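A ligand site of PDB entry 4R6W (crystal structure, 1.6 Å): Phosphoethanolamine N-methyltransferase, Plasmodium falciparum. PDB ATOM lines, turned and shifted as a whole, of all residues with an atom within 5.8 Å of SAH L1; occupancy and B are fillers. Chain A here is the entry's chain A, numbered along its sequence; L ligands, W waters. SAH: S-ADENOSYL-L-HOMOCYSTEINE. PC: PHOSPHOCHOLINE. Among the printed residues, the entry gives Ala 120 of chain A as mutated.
Residues that only touch SAH L1: Leu 6 (3.7 Å), Tyr 27 (3.8 Å), Ser 56 (3.9 Å), Gly 57 (3.7 Å), Ile 82 (3.4 Å), Asn 101 (3.6 Å), Ala 120 (3.5 Å), Ala 121 (3.4 Å), His 124 (3.7 Å) and Leu 125 (3.9 Å). Hydrophobic or aromatic side chains within 4 Å of SAH L1: Leu 6, Tyr 11, Ile 28, Ile 78, Ile 82, Ile 103, Ala 121, His 124 and Leu 125. 20 residues have an atom within 4 Å of SAH L1: Leu 6, Tyr 11, Tyr 27, Ile 28, Ser 29, Gly 55, Ser 56, Gly 57, Asp 77, Ile 78, Cys 79, Ile 82, Asn 101, Asp 102, Ile 103, Arg 119, Ala 120, Ala 121, His 124 and Leu 125.
The backbone NH of Asn 101 is in hydrogen-bond range of the backbone carbonyl oxygen of Asp 77 (2.9 Å). N of Ser 56 lies within hydrogen-bond range of OD2 of Asp 77, 3.5 Å away. The backbone NH of Gly 57 lies within hydrogen-bond range of the side-chain carboxylate of Asp 77, 2.9 Å away. N of Tyr 11 is in hydrogen-bond range of O of Leu 6 (2.9 Å). The side-chain hydroxyl (OH) of Tyr 11 is in hydrogen-bond range of a ring nitrogen (NE2) of His 124 (2.8 Å). The backbone NH (N) of Cys 79 sits at hydrogen-bond distance from the side-chain carboxylate (OD1) of Asp 77 (3.0 Å). N of Gly 55 is in hydrogen-bond range of O of Ile 76 (2.7 Å). N of Ser 56 sits at hydrogen-bond distance from O of Ile 76.
Water W1 lies within hydrogen-bond range of an oxygen (OXT) of SAH L1, the backbone carbonyl oxygen of Asn 26 and the backbone NH of Leu 58. Water W2 bridges N of SAH L1 and OD2 of Asp 53. Water W5 lies within hydrogen-bond range of an oxygen (O) of SAH L1 (2.9 Å), the side-chain hydroxyl (OG) of Ser 29 (3.1 Å) and the guanidinium group (NH1) of Arg 119 (3.2 Å).
The backbone carbonyl oxygen (O) of Gly 55 sits at hydrogen-bond distance from a nitrogen (N) of SAH L1, 2.8 Å away. N3 of SAH L1 is in hydrogen-bond range of N of Ile 78 (3.2 Å). The side-chain carboxylate (OD1) of Asp 102 lies within hydrogen-bond range of a nitrogen (N6) of SAH L1 (2.9 Å). A nitrogen (N) of SAH L1 lies within hydrogen-bond range of the backbone carbonyl oxygen of Arg 119 (2.9 Å). OG of Ser 29 lies within hydrogen-bond range of O of SAH L1 (2.6 Å). SD of SAH L1 sits close to OH of Tyr 11, at 3.7 Å. SG of Cys 79 is in hydrogen-bond range of O2' of SAH L1 (3.4 Å). The side-chain carboxylate (OD1) of Asp 77 sits at hydrogen-bond distance from an oxygen (O2') of SAH L1, at 2.5 Å. The backbone NH (N) of Ile 28 sits at hydrogen-bond distance from an oxygen (OXT) of SAH L1 (2.8 Å). N of Ile 103 sits at hydrogen-bond distance from N1 of SAH L1 (3.0 Å).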
ATOM      1  N   LEU A   6     -19.693 -24.396  -6.845  1.00  0.00           N
ATOM      2  CA  LEU A   6     -18.263 -24.244  -6.641  1.00  0.00           C
ATOM      3  C   LEU A   6     -17.937 -23.413  -5.394  1.00  0.00           C
ATOM      4  O   LEU A   6     -17.057 -23.780  -4.610  1.00  0.00           O
ATOM      5  CB  LEU A   6     -17.620 -23.625  -7.884  1.00  0.00           C
ATOM      6  CG  LEU A   6     -17.709 -24.485  -9.142  1.00  0.00           C
ATOM      7  CD1 LEU A   6     -17.200 -23.689 -10.327  1.00  0.00           C
ATOM      8  CD2 LEU A   6     -16.905 -25.777  -8.988  1.00  0.00           C
ATOM      9  N   TYR A  11     -14.534 -24.734  -3.626  1.00  0.00           N
ATOM     10  CA  TYR A  11     -13.799 -23.489  -3.520  1.00  0.00           C
ATOM     11  C   TYR A  11     -14.440 -22.540  -2.513  1.00  0.00           C
ATOM     12  O   TYR A  11     -14.568 -21.333  -2.747  1.00  0.00           O
ATOM     13  CB  TYR A  11     -13.684 -22.818  -4.896  1.00  0.00           C
ATOM     14  CG  TYR A  11     -13.021 -23.694  -5.951  1.00  0.00           C
ATOM     15  CD1 TYR A  11     -11.704 -24.103  -5.814  1.00  0.00           C
ATOM     16  CD2 TYR A  11     -13.719 -24.105  -7.081  1.00  0.00           C
ATOM     17  CE1 TYR A  11     -11.097 -24.901  -6.786  1.00  0.00           C
ATOM     18  CE2 TYR A  11     -13.121 -24.899  -8.057  1.00  0.00           C
ATOM     19  CZ  TYR A  11     -11.808 -25.289  -7.896  1.00  0.00           C
ATOM     20  OH  TYR A  11     -11.185 -26.078  -8.847  1.00  0.00           O
ATOM     21  N   ASN A  26      -0.671 -18.088  -3.823  1.00  0.00           N
ATOM     22  CA  ASN A  26      -1.395 -17.553  -4.984  1.00  0.00           C
ATOM     23  C   ASN A  26      -1.788 -18.587  -6.029  1.00  0.00           C
ATOM     24  O   ASN A  26      -2.255 -18.211  -7.097  1.00  0.00           O
ATOM     25  CB  ASN A  26      -0.602 -16.442  -5.695  1.00  0.00           C
ATOM     26  CG  ASN A  26      -0.162 -15.334  -4.767  1.00  0.00           C
ATOM     27  OD1 ASN A  26      -0.923 -14.890  -3.899  1.00  0.00           O
ATOM     28  ND2 ASN A  26       1.069 -14.874  -4.935  1.00  0.00           N
ATOM     29  N   TYR A  27      -1.627 -19.877  -5.722  1.00  0.00           N
ATOM     30  CA  TYR A  27      -1.962 -20.927  -6.683  1.00  0.00           C
ATOM     31  C   TYR A  27      -2.992 -21.915  -6.134  1.00  0.00           C
ATOM     32  O   TYR A  27      -3.029 -22.176  -4.937  1.00  0.00           O
ATOM     33  CB  TYR A  27      -0.690 -21.660  -7.107  1.00  0.00           C
ATOM     34  CG  TYR A  27       0.141 -20.830  -8.062  1.00  0.00           C
ATOM     35  CD1 TYR A  27      -0.136 -20.833  -9.422  1.00  0.00           C
ATOM     36  CD2 TYR A  27       1.163 -20.021  -7.587  1.00  0.00           C
ATOM     37  CE1 TYR A  27       0.604 -20.065 -10.306  1.00  0.00           C
ATOM     38  CE2 TYR A  27       1.904 -19.246  -8.465  1.00  0.00           C
ATOM     39  CZ  TYR A  27       1.622 -19.278  -9.819  1.00  0.00           C
ATOM     40  OH  TYR A  27       2.347 -18.519 -10.707  1.00  0.00           O
ATOM     41  N   ILE A  28      -3.803 -22.459  -7.050  1.00  0.00           N
ATOM     42  CA  ILE A  28      -4.753 -23.526  -6.716  1.00  0.00           C
ATOM     43  C   ILE A  28      -4.567 -24.709  -7.668  1.00  0.00           C
ATOM     44  O   ILE A  28      -5.490 -25.485  -7.914  1.00  0.00           O
ATOM     45  CB  ILE A  28      -6.237 -23.065  -6.794  1.00  0.00           C
ATOM     46  CG1 ILE A  28      -6.403 -21.573  -6.461  1.00  0.00           C
ATOM     47  CG2 ILE A  28      -7.105 -23.902  -5.845  1.00  0.00           C
ATOM     48  CD1 ILE A  28      -7.881 -21.105  -6.499  1.00  0.00           C
ATOM     49  N   SER A  29      -3.376 -24.844  -8.227  1.00  0.00           N
ATOM     50  CA  SER A  29      -3.111 -26.006  -9.080  1.00  0.00           C
ATOM     51  C   SER A  29      -1.641 -26.406  -9.015  1.00  0.00           C
ATOM     52  O   SER A  29      -0.797 -25.660  -8.512  1.00  0.00           O
ATOM     53  CB  SER A  29      -3.557 -25.743 -10.513  1.00  0.00           C
ATOM     54  OG  SER A  29      -2.720 -24.815 -11.168  1.00  0.00           O
ATOM     55  N   ASP A  53      -6.822 -14.848 -18.869  1.00  0.00           N
ATOM     56  CA  ASP A  53      -6.640 -16.039 -18.035  1.00  0.00           C
ATOM     57  C   ASP A  53      -8.016 -16.577 -17.641  1.00  0.00           C
ATOM     58  O   ASP A  53      -8.731 -15.954 -16.844  1.00  0.00           O
ATOM     59  CB  ASP A  53      -5.822 -15.728 -16.783  1.00  0.00           C
ATOM     60  CG  ASP A  53      -5.470 -16.969 -15.943  1.00  0.00           C
ATOM     61  OD1 ASP A  53      -6.057 -18.055 -16.167  1.00  0.00           O
ATOM     62  OD2 ASP A  53      -4.620 -16.853 -15.031  1.00  0.00           O
ATOM     63  N   ILE A  54      -8.371 -17.725 -18.192  1.00  0.00           N
ATOM     64  CA  ILE A  54      -9.675 -18.326 -17.917  1.00  0.00           C
ATOM     65  C   ILE A  54      -9.615 -19.197 -16.671  1.00  0.00           C
ATOM     66  O   ILE A  54      -8.935 -20.222 -16.627  1.00  0.00           O
ATOM     67  CB  ILE A  54     -10.185 -19.168 -19.105  1.00  0.00           C
ATOM     68  CG1 ILE A  54     -10.316 -18.302 -20.358  1.00  0.00           C
ATOM     69  CG2 ILE A  54     -11.522 -19.852 -18.769  1.00  0.00           C
ATOM     70  CD1 ILE A  54     -10.700 -19.051 -21.610  1.00  0.00           C
ATOM     71  N   GLY A  55     -10.341 -18.771 -15.634  1.00  0.00           N
ATOM     72  CA  GLY A  55     -10.278 -19.438 -14.357  1.00  0.00           C
ATOM     73  C   GLY A  55      -9.064 -18.992 -13.569  1.00  0.00           C
ATOM     74  O   GLY A  55      -8.251 -19.830 -13.154  1.00  0.00           O
ATOM     75  N   SER A  56      -8.953 -17.693 -13.346  1.00  0.00           N
ATOM     76  CA  SER A  56      -7.726 -17.091 -12.812  1.00  0.00           C
ATOM     77  C   SER A  56      -7.415 -17.382 -11.334  1.00  0.00           C
ATOM     78  O   SER A  56      -6.292 -17.158 -10.908  1.00  0.00           O
ATOM     79  CB  SER A  56      -7.757 -15.570 -13.050  1.00  0.00           C
ATOM     80  OG  SER A  56      -9.018 -15.009 -12.681  1.00  0.00           O
ATOM     81  N   GLY A  57      -8.381 -17.881 -10.573  1.00  0.00           N
ATOM     82  CA  GLY A  57      -8.120 -18.285  -9.190  1.00  0.00           C
ATOM     83  C   GLY A  57      -7.607 -17.167  -8.297  1.00  0.00           C
ATOM     84  O   GLY A  57      -8.147 -16.065  -8.285  1.00  0.00           O
ATOM     85  N   LEU A  58      -6.543 -17.467  -7.546  1.00  0.00           N
ATOM     86  CA  LEU A  58      -5.953 -16.487  -6.642  1.00  0.00           C
ATOM     87  C   LEU A  58      -5.028 -15.526  -7.362  1.00  0.00           C
ATOM     88  O   LEU A  58      -4.471 -14.629  -6.742  1.00  0.00           O
ATOM     89  CB  LEU A  58      -5.182 -17.196  -5.536  1.00  0.00           C
ATOM     90  CG  LEU A  58      -6.040 -18.005  -4.557  1.00  0.00           C
ATOM     91  CD1 LEU A  58      -5.151 -18.753  -3.589  1.00  0.00           C
ATOM     92  CD2 LEU A  58      -6.971 -17.076  -3.802  1.00  0.00           C
ATOM     93  N   ILE A  76     -10.553 -14.036 -15.496  1.00  0.00           N
ATOM     94  CA  ILE A  76     -11.972 -14.253 -15.270  1.00  0.00           C
ATOM     95  C   ILE A  76     -12.133 -15.473 -14.392  1.00  0.00           C
ATOM     96  O   ILE A  76     -11.561 -16.531 -14.677  1.00  0.00           O
ATOM     97  CB  ILE A  76     -12.737 -14.475 -16.592  1.00  0.00           C
ATOM     98  CG1 ILE A  76     -12.632 -13.245 -17.496  1.00  0.00           C
ATOM     99  CG2 ILE A  76     -14.210 -14.759 -16.325  1.00  0.00           C
ATOM    100  CD1 ILE A  76     -13.529 -12.094 -17.048  1.00  0.00           C
ATOM    101  N   ASP A  77     -12.903 -15.339 -13.318  1.00  0.00           N
ATOM    102  CA  ASP A  77     -13.181 -16.496 -12.465  1.00  0.00           C
ATOM    103  C   ASP A  77     -14.628 -16.431 -12.014  1.00  0.00           C
ATOM    104  O   ASP A  77     -15.136 -15.356 -11.721  1.00  0.00           O
ATOM    105  CB  ASP A  77     -12.242 -16.535 -11.257  1.00  0.00           C
ATOM    106  CG  ASP A  77     -12.186 -17.902 -10.614  1.00  0.00           C
ATOM    107  OD1 ASP A  77     -13.156 -18.275  -9.900  1.00  0.00           O
ATOM    108  OD2 ASP A  77     -11.179 -18.625 -10.853  1.00  0.00           O
ATOM    109  N   ILE A  78     -15.300 -17.581 -11.951  1.00  0.00           N
ATOM    110  CA  ILE A  78     -16.732 -17.577 -11.650  1.00  0.00           C
ATOM    111  C   ILE A  78     -17.024 -17.419 -10.144  1.00  0.00           C
ATOM    112  O   ILE A  78     -18.101 -16.969  -9.757  1.00  0.00           O
ATOM    113  CB  ILE A  78     -17.412 -18.867 -12.194  1.00  0.00           C
ATOM    114  CG1 ILE A  78     -18.940 -18.690 -12.229  1.00  0.00           C
ATOM    115  CG2 ILE A  78     -16.991 -20.097 -11.407  1.00  0.00           C
ATOM    116  CD1 ILE A  78     -19.667 -19.817 -12.982  1.00  0.00           C
ATOM    117  N   CYS A  79     -16.057 -17.770  -9.304  1.00  0.00           N
ATOM    118  CA  CYS A  79     -16.259 -17.705  -7.863  1.00  0.00           C
ATOM    119  C   CYS A  79     -15.935 -16.329  -7.309  1.00  0.00           C
ATOM    120  O   CYS A  79     -14.777 -15.912  -7.286  1.00  0.00           O
ATOM    121  CB  CYS A  79     -15.405 -18.762  -7.164  1.00  0.00           C
ATOM    122  SG  CYS A  79     -15.985 -20.459  -7.446  1.00  0.00           S
ATOM    123  N   ILE A  82     -13.345 -16.043  -4.494  1.00  0.00           N
ATOM    124  CA  ILE A  82     -11.965 -16.240  -4.933  1.00  0.00           C
ATOM    125  C   ILE A  82     -11.443 -14.965  -5.594  1.00  0.00           C
ATOM    126  O   ILE A  82     -10.314 -14.540  -5.348  1.00  0.00           O
ATOM    127  CB  ILE A  82     -11.831 -17.408  -5.935  1.00  0.00           C
ATOM    128  CG1 ILE A  82     -12.207 -18.739  -5.278  1.00  0.00           C
ATOM    129  CG2 ILE A  82     -10.418 -17.484  -6.469  1.00  0.00           C
ATOM    130  CD1 ILE A  82     -12.042 -19.912  -6.226  1.00  0.00           C
ATOM    131  N   ASN A 101     -16.990 -13.611 -13.137  1.00  0.00           N
ATOM    132  CA  ASN A 101     -17.935 -13.886 -14.215  1.00  0.00           C
ATOM    133  C   ASN A 101     -17.808 -15.326 -14.681  1.00  0.00           C
ATOM    134  O   ASN A 101     -16.739 -15.923 -14.563  1.00  0.00           O
ATOM    135  CB  ASN A 101     -17.701 -12.926 -15.384  1.00  0.00           C
ATOM    136  CG  ASN A 101     -18.985 -12.378 -15.966  1.00  0.00           C
ATOM    137  OD1 ASN A 101     -19.868 -13.126 -16.398  1.00  0.00           O
ATOM    138  ND2 ASN A 101     -19.108 -11.055 -15.974  1.00  0.00           N
ATOM    139  N   ASP A 102     -18.896 -15.861 -15.212  1.00  0.00           N
ATOM    140  CA  ASP A 102     -18.888 -17.129 -15.928  1.00  0.00           C
ATOM    141  C   ASP A 102     -18.260 -16.878 -17.298  1.00  0.00           C
ATOM    142  O   ASP A 102     -18.745 -16.016 -18.030  1.00  0.00           O
ATOM    143  CB  ASP A 102     -20.312 -17.666 -16.058  1.00  0.00           C
ATOM    144  CG  ASP A 102     -20.400 -19.034 -16.702  1.00  0.00           C
ATOM    145  OD1 ASP A 102     -19.380 -19.569 -17.171  1.00  0.00           O
ATOM    146  OD2 ASP A 102     -21.523 -19.586 -16.748  1.00  0.00           O
ATOM    147  N   ILE A 103     -17.204 -17.622 -17.646  1.00  0.00           N
ATOM    148  CA  ILE A 103     -16.554 -17.386 -18.933  1.00  0.00           C
ATOM    149  C   ILE A 103     -17.501 -17.710 -20.095  1.00  0.00           C
ATOM    150  O   ILE A 103     -17.361 -17.172 -21.199  1.00  0.00           O
ATOM    151  CB  ILE A 103     -15.243 -18.212 -19.074  1.00  0.00           C
ATOM    152  CG1 ILE A 103     -14.428 -17.755 -20.298  1.00  0.00           C
ATOM    153  CG2 ILE A 103     -15.540 -19.705 -19.115  1.00  0.00           C
ATOM    154  CD1 ILE A 103     -13.912 -16.333 -20.179  1.00  0.00           C
ATOM    155  N   LEU A 104     -18.496 -18.547 -19.844  1.00  0.00           N
ATOM    156  CA  LEU A 104     -19.419 -18.956 -20.896  1.00  0.00           C
ATOM    157  C   LEU A 104     -20.388 -17.839 -21.304  1.00  0.00           C
ATOM    158  O   LEU A 104     -20.944 -17.877 -22.402  1.00  0.00           O
ATOM    159  CB  LEU A 104     -20.210 -20.198 -20.459  1.00  0.00           C
ATOM    160  CG  LEU A 104     -19.360 -21.466 -20.324  1.00  0.00           C
ATOM    161  CD1 LEU A 104     -20.170 -22.580 -19.675  1.00  0.00           C
ATOM    162  CD2 LEU A 104     -18.813 -21.889 -21.665  1.00  0.00           C
ATOM    163  N   SER A 118      -5.146 -20.933 -19.725  1.00  0.00           N
ATOM    164  CA  SER A 118      -6.022 -21.528 -18.712  1.00  0.00           C
ATOM    165  C   SER A 118      -5.326 -22.692 -18.062  1.00  0.00           C
ATOM    166  O   SER A 118      -4.722 -23.515 -18.753  1.00  0.00           O
ATOM    167  CB  SER A 118      -7.344 -21.977 -19.325  1.00  0.00           C
ATOM    168  OG  SER A 118      -8.248 -22.394 -18.313  1.00  0.00           O
ATOM    169  N   ARG A 119      -5.379 -22.759 -16.738  1.00  0.00           N
ATOM    170  CA  ARG A 119      -4.697 -23.809 -15.987  1.00  0.00           C
ATOM    171  C   ARG A 119      -5.702 -24.431 -15.030  1.00  0.00           C
ATOM    172  O   ARG A 119      -6.187 -23.765 -14.124  1.00  0.00           O
ATOM    173  CB  ARG A 119      -3.513 -23.247 -15.201  1.00  0.00           C
ATOM    174  CG  ARG A 119      -2.509 -22.471 -16.047  1.00  0.00           C
ATOM    175  CD  ARG A 119      -1.597 -23.400 -16.834  1.00  0.00           C
ATOM    176  NE  ARG A 119      -1.032 -24.404 -15.939  1.00  0.00           N
ATOM    177  CZ  ARG A 119      -0.030 -24.176 -15.101  1.00  0.00           C
ATOM    178  NH1 ARG A 119       0.556 -22.979 -15.054  1.00  0.00           N
ATOM    179  NH2 ARG A 119       0.395 -25.148 -14.305  1.00  0.00           N
ATOM    180  N   ALA A 120      -6.028 -25.698 -15.280  1.00  0.00           N
ATOM    181  CA  ALA A 120      -6.848 -26.506 -14.373  1.00  0.00           C
ATOM    182  C   ALA A 120      -8.210 -25.915 -14.086  1.00  0.00           C
ATOM    183  O   ALA A 120      -8.661 -25.963 -12.942  1.00  0.00           O
ATOM    184  CB  ALA A 120      -6.092 -26.735 -13.053  1.00  0.00           C
ATOM    185  N   ALA A 121      -8.876 -25.394 -15.116  1.00  0.00           N
ATOM    186  CA  ALA A 121     -10.194 -24.775 -14.935  1.00  0.00           C
ATOM    187  C   ALA A 121     -11.280 -25.388 -15.809  1.00  0.00           C
ATOM    188  O   ALA A 121     -12.449 -25.483 -15.397  1.00  0.00           O
ATOM    189  CB  ALA A 121     -10.100 -23.269 -15.211  1.00  0.00           C
ATOM    190  N   LEU A 123     -11.792 -28.382 -16.806  1.00  0.00           N
ATOM    191  CA  LEU A 123     -12.372 -29.627 -16.264  1.00  0.00           C
ATOM    192  C   LEU A 123     -13.757 -29.433 -15.589  1.00  0.00           C
ATOM    193  O   LEU A 123     -14.544 -30.376 -15.477  1.00  0.00           O
ATOM    194  CB  LEU A 123     -11.405 -30.253 -15.246  1.00  0.00           C
ATOM    195  CG  LEU A 123     -11.342 -29.665 -13.829  1.00  0.00           C
ATOM    196  CD1 LEU A 123     -10.556 -30.586 -12.909  1.00  0.00           C
ATOM    197  CD2 LEU A 123     -10.736 -28.268 -13.831  1.00  0.00           C
ATOM    198  N   HIS A 124     -14.076 -28.208 -15.176  1.00  0.00           N
ATOM    199  CA  HIS A 124     -15.358 -27.940 -14.539  1.00  0.00           C
ATOM    200  C   HIS A 124     -16.504 -27.846 -15.541  1.00  0.00           C
ATOM    201  O   HIS A 124     -17.681 -27.923 -15.169  1.00  0.00           O
ATOM    202  CB  HIS A 124     -15.281 -26.646 -13.732  1.00  0.00           C
ATOM    203  CG  HIS A 124     -14.431 -26.751 -12.482  1.00  0.00           C
ATOM    204  ND1 HIS A 124     -14.807 -27.514 -11.429  1.00  0.00           N
ATOM    205  CD2 HIS A 124     -13.256 -26.157 -12.180  1.00  0.00           C
ATOM    206  CE1 HIS A 124     -13.868 -27.407 -10.462  1.00  0.00           C
ATOM    207  NE2 HIS A 124     -12.936 -26.610 -10.902  1.00  0.00           N
ATOM    208  N   LEU A 125     -16.171 -27.669 -16.813  1.00  0.00           N
ATOM    209  CA  LEU A 125     -17.160 -27.489 -17.873  1.00  0.00           C
ATOM    210  C   LEU A 125     -17.638 -28.816 -18.464  1.00  0.00           C
ATOM    211  O   LEU A 125     -16.853 -29.737 -18.662  1.00  0.00           O
ATOM    212  CB  LEU A 125     -16.588 -26.603 -18.983  1.00  0.00           C
ATOM    213  CG  LEU A 125     -16.728 -25.083 -18.834  1.00  0.00           C
ATOM    214  CD1 LEU A 125     -16.030 -24.564 -17.566  1.00  0.00           C
ATOM    215  CD2 LEU A 125     -16.192 -24.365 -20.068  1.00  0.00           C
HETATM  216  N   SAH L   1      -5.765 -21.164 -12.839  1.00  0.00           N
HETATM  217  CA  SAH L   1      -5.611 -21.011 -11.372  1.00  0.00           C
HETATM  218  CB  SAH L   1      -6.941 -21.430 -10.641  1.00  0.00           C
HETATM  219  CG  SAH L   1      -7.317 -22.897 -10.808  1.00  0.00           C
HETATM  220  SD  SAH L   1      -8.785 -23.382  -9.852  1.00  0.00           S
HETATM  221  C   SAH L   1      -4.430 -21.748 -10.897  1.00  0.00           C
HETATM  222  O   SAH L   1      -3.904 -22.575 -11.628  1.00  0.00           O
HETATM  223  OXT SAH L   1      -4.047 -21.609  -9.755  1.00  0.00           O
HETATM  224  C5' SAH L   1     -10.163 -23.427 -11.020  1.00  0.00           C
HETATM  225  C4' SAH L   1     -10.798 -22.173 -11.251  1.00  0.00           C
HETATM  226  O4' SAH L   1     -11.691 -22.294 -12.384  1.00  0.00           O
HETATM  227  C3' SAH L   1     -11.647 -21.901 -10.070  1.00  0.00           C
HETATM  228  O3' SAH L   1     -11.169 -20.745  -9.422  1.00  0.00           O
HETATM  229  C2' SAH L   1     -13.010 -21.746 -10.613  1.00  0.00           C
HETATM  230  O2' SAH L   1     -13.710 -20.706  -9.968  1.00  0.00           O
HETATM  231  C1' SAH L   1     -12.785 -21.486 -12.069  1.00  0.00           C
HETATM  232  N9  SAH L   1     -13.995 -21.764 -12.928  1.00  0.00           N
HETATM  233  C8  SAH L   1     -14.710 -22.883 -12.985  1.00  0.00           C
HETATM  234  N7  SAH L   1     -15.686 -22.717 -13.878  1.00  0.00           N
HETATM  235  C5  SAH L   1     -15.598 -21.478 -14.398  1.00  0.00           C
HETATM  236  C6  SAH L   1     -16.344 -20.782 -15.356  1.00  0.00           C
HETATM  237  N6  SAH L   1     -17.449 -21.328 -15.955  1.00  0.00           N
HETATM  238  N1  SAH L   1     -15.968 -19.523 -15.642  1.00  0.00           N
HETATM  239  C2  SAH L   1     -14.901 -18.959 -15.047  1.00  0.00           C
HETATM  240  N3  SAH L   1     -14.161 -19.613 -14.110  1.00  0.00           N
HETATM  241  C4  SAH L   1     -14.504 -20.872 -13.795  1.00  0.00           C
HETATM  242  P1   PC L   2      -8.484 -31.858  -6.828  1.00  0.00           P
HETATM  243  O1   PC L   2      -9.596 -32.617  -7.527  1.00  0.00           O
HETATM  244  O3   PC L   2      -8.566 -31.841  -5.332  1.00  0.00           O
HETATM  245  O4   PC L   2      -7.158 -32.331  -7.333  1.00  0.00           O
HETATM  246  O2   PC L   2      -8.626 -30.384  -7.377  1.00  0.00           O
HETATM  247  C1   PC L   2      -7.625 -29.416  -7.091  1.00  0.00           C
HETATM  248  C2   PC L   2      -7.884 -28.055  -7.748  1.00  0.00           C
HETATM  249  N1   PC L   2      -7.807 -27.991  -9.233  1.00  0.00           N
HETATM  250  C3   PC L   2      -6.441 -28.510  -9.647  1.00  0.00           C
HETATM  251  C4   PC L   2      -8.084 -26.632  -9.606  1.00  0.00           C
HETATM  252  C5   PC L   2      -8.800 -28.757  -9.865  1.00  0.00           C
HETATM  253  O   HOH W   1      -4.447 -19.191  -8.622  1.00  0.00           O
HETATM  254  O   HOH W   2      -3.764 -19.297 -13.675  1.00  0.00           O
HETATM  255  O   HOH W   3      -3.376 -18.331 -11.145  1.00  0.00           O
HETATM  256  O   HOH W   4      -6.418 -20.402 -15.403  1.00  0.00           O
HETATM  257  O   HOH W   5      -1.119 -22.436 -12.416  1.00  0.00           O
HETATM  258  O   HOH W   6     -18.105 -24.144 -14.264  1.00  0.00           O
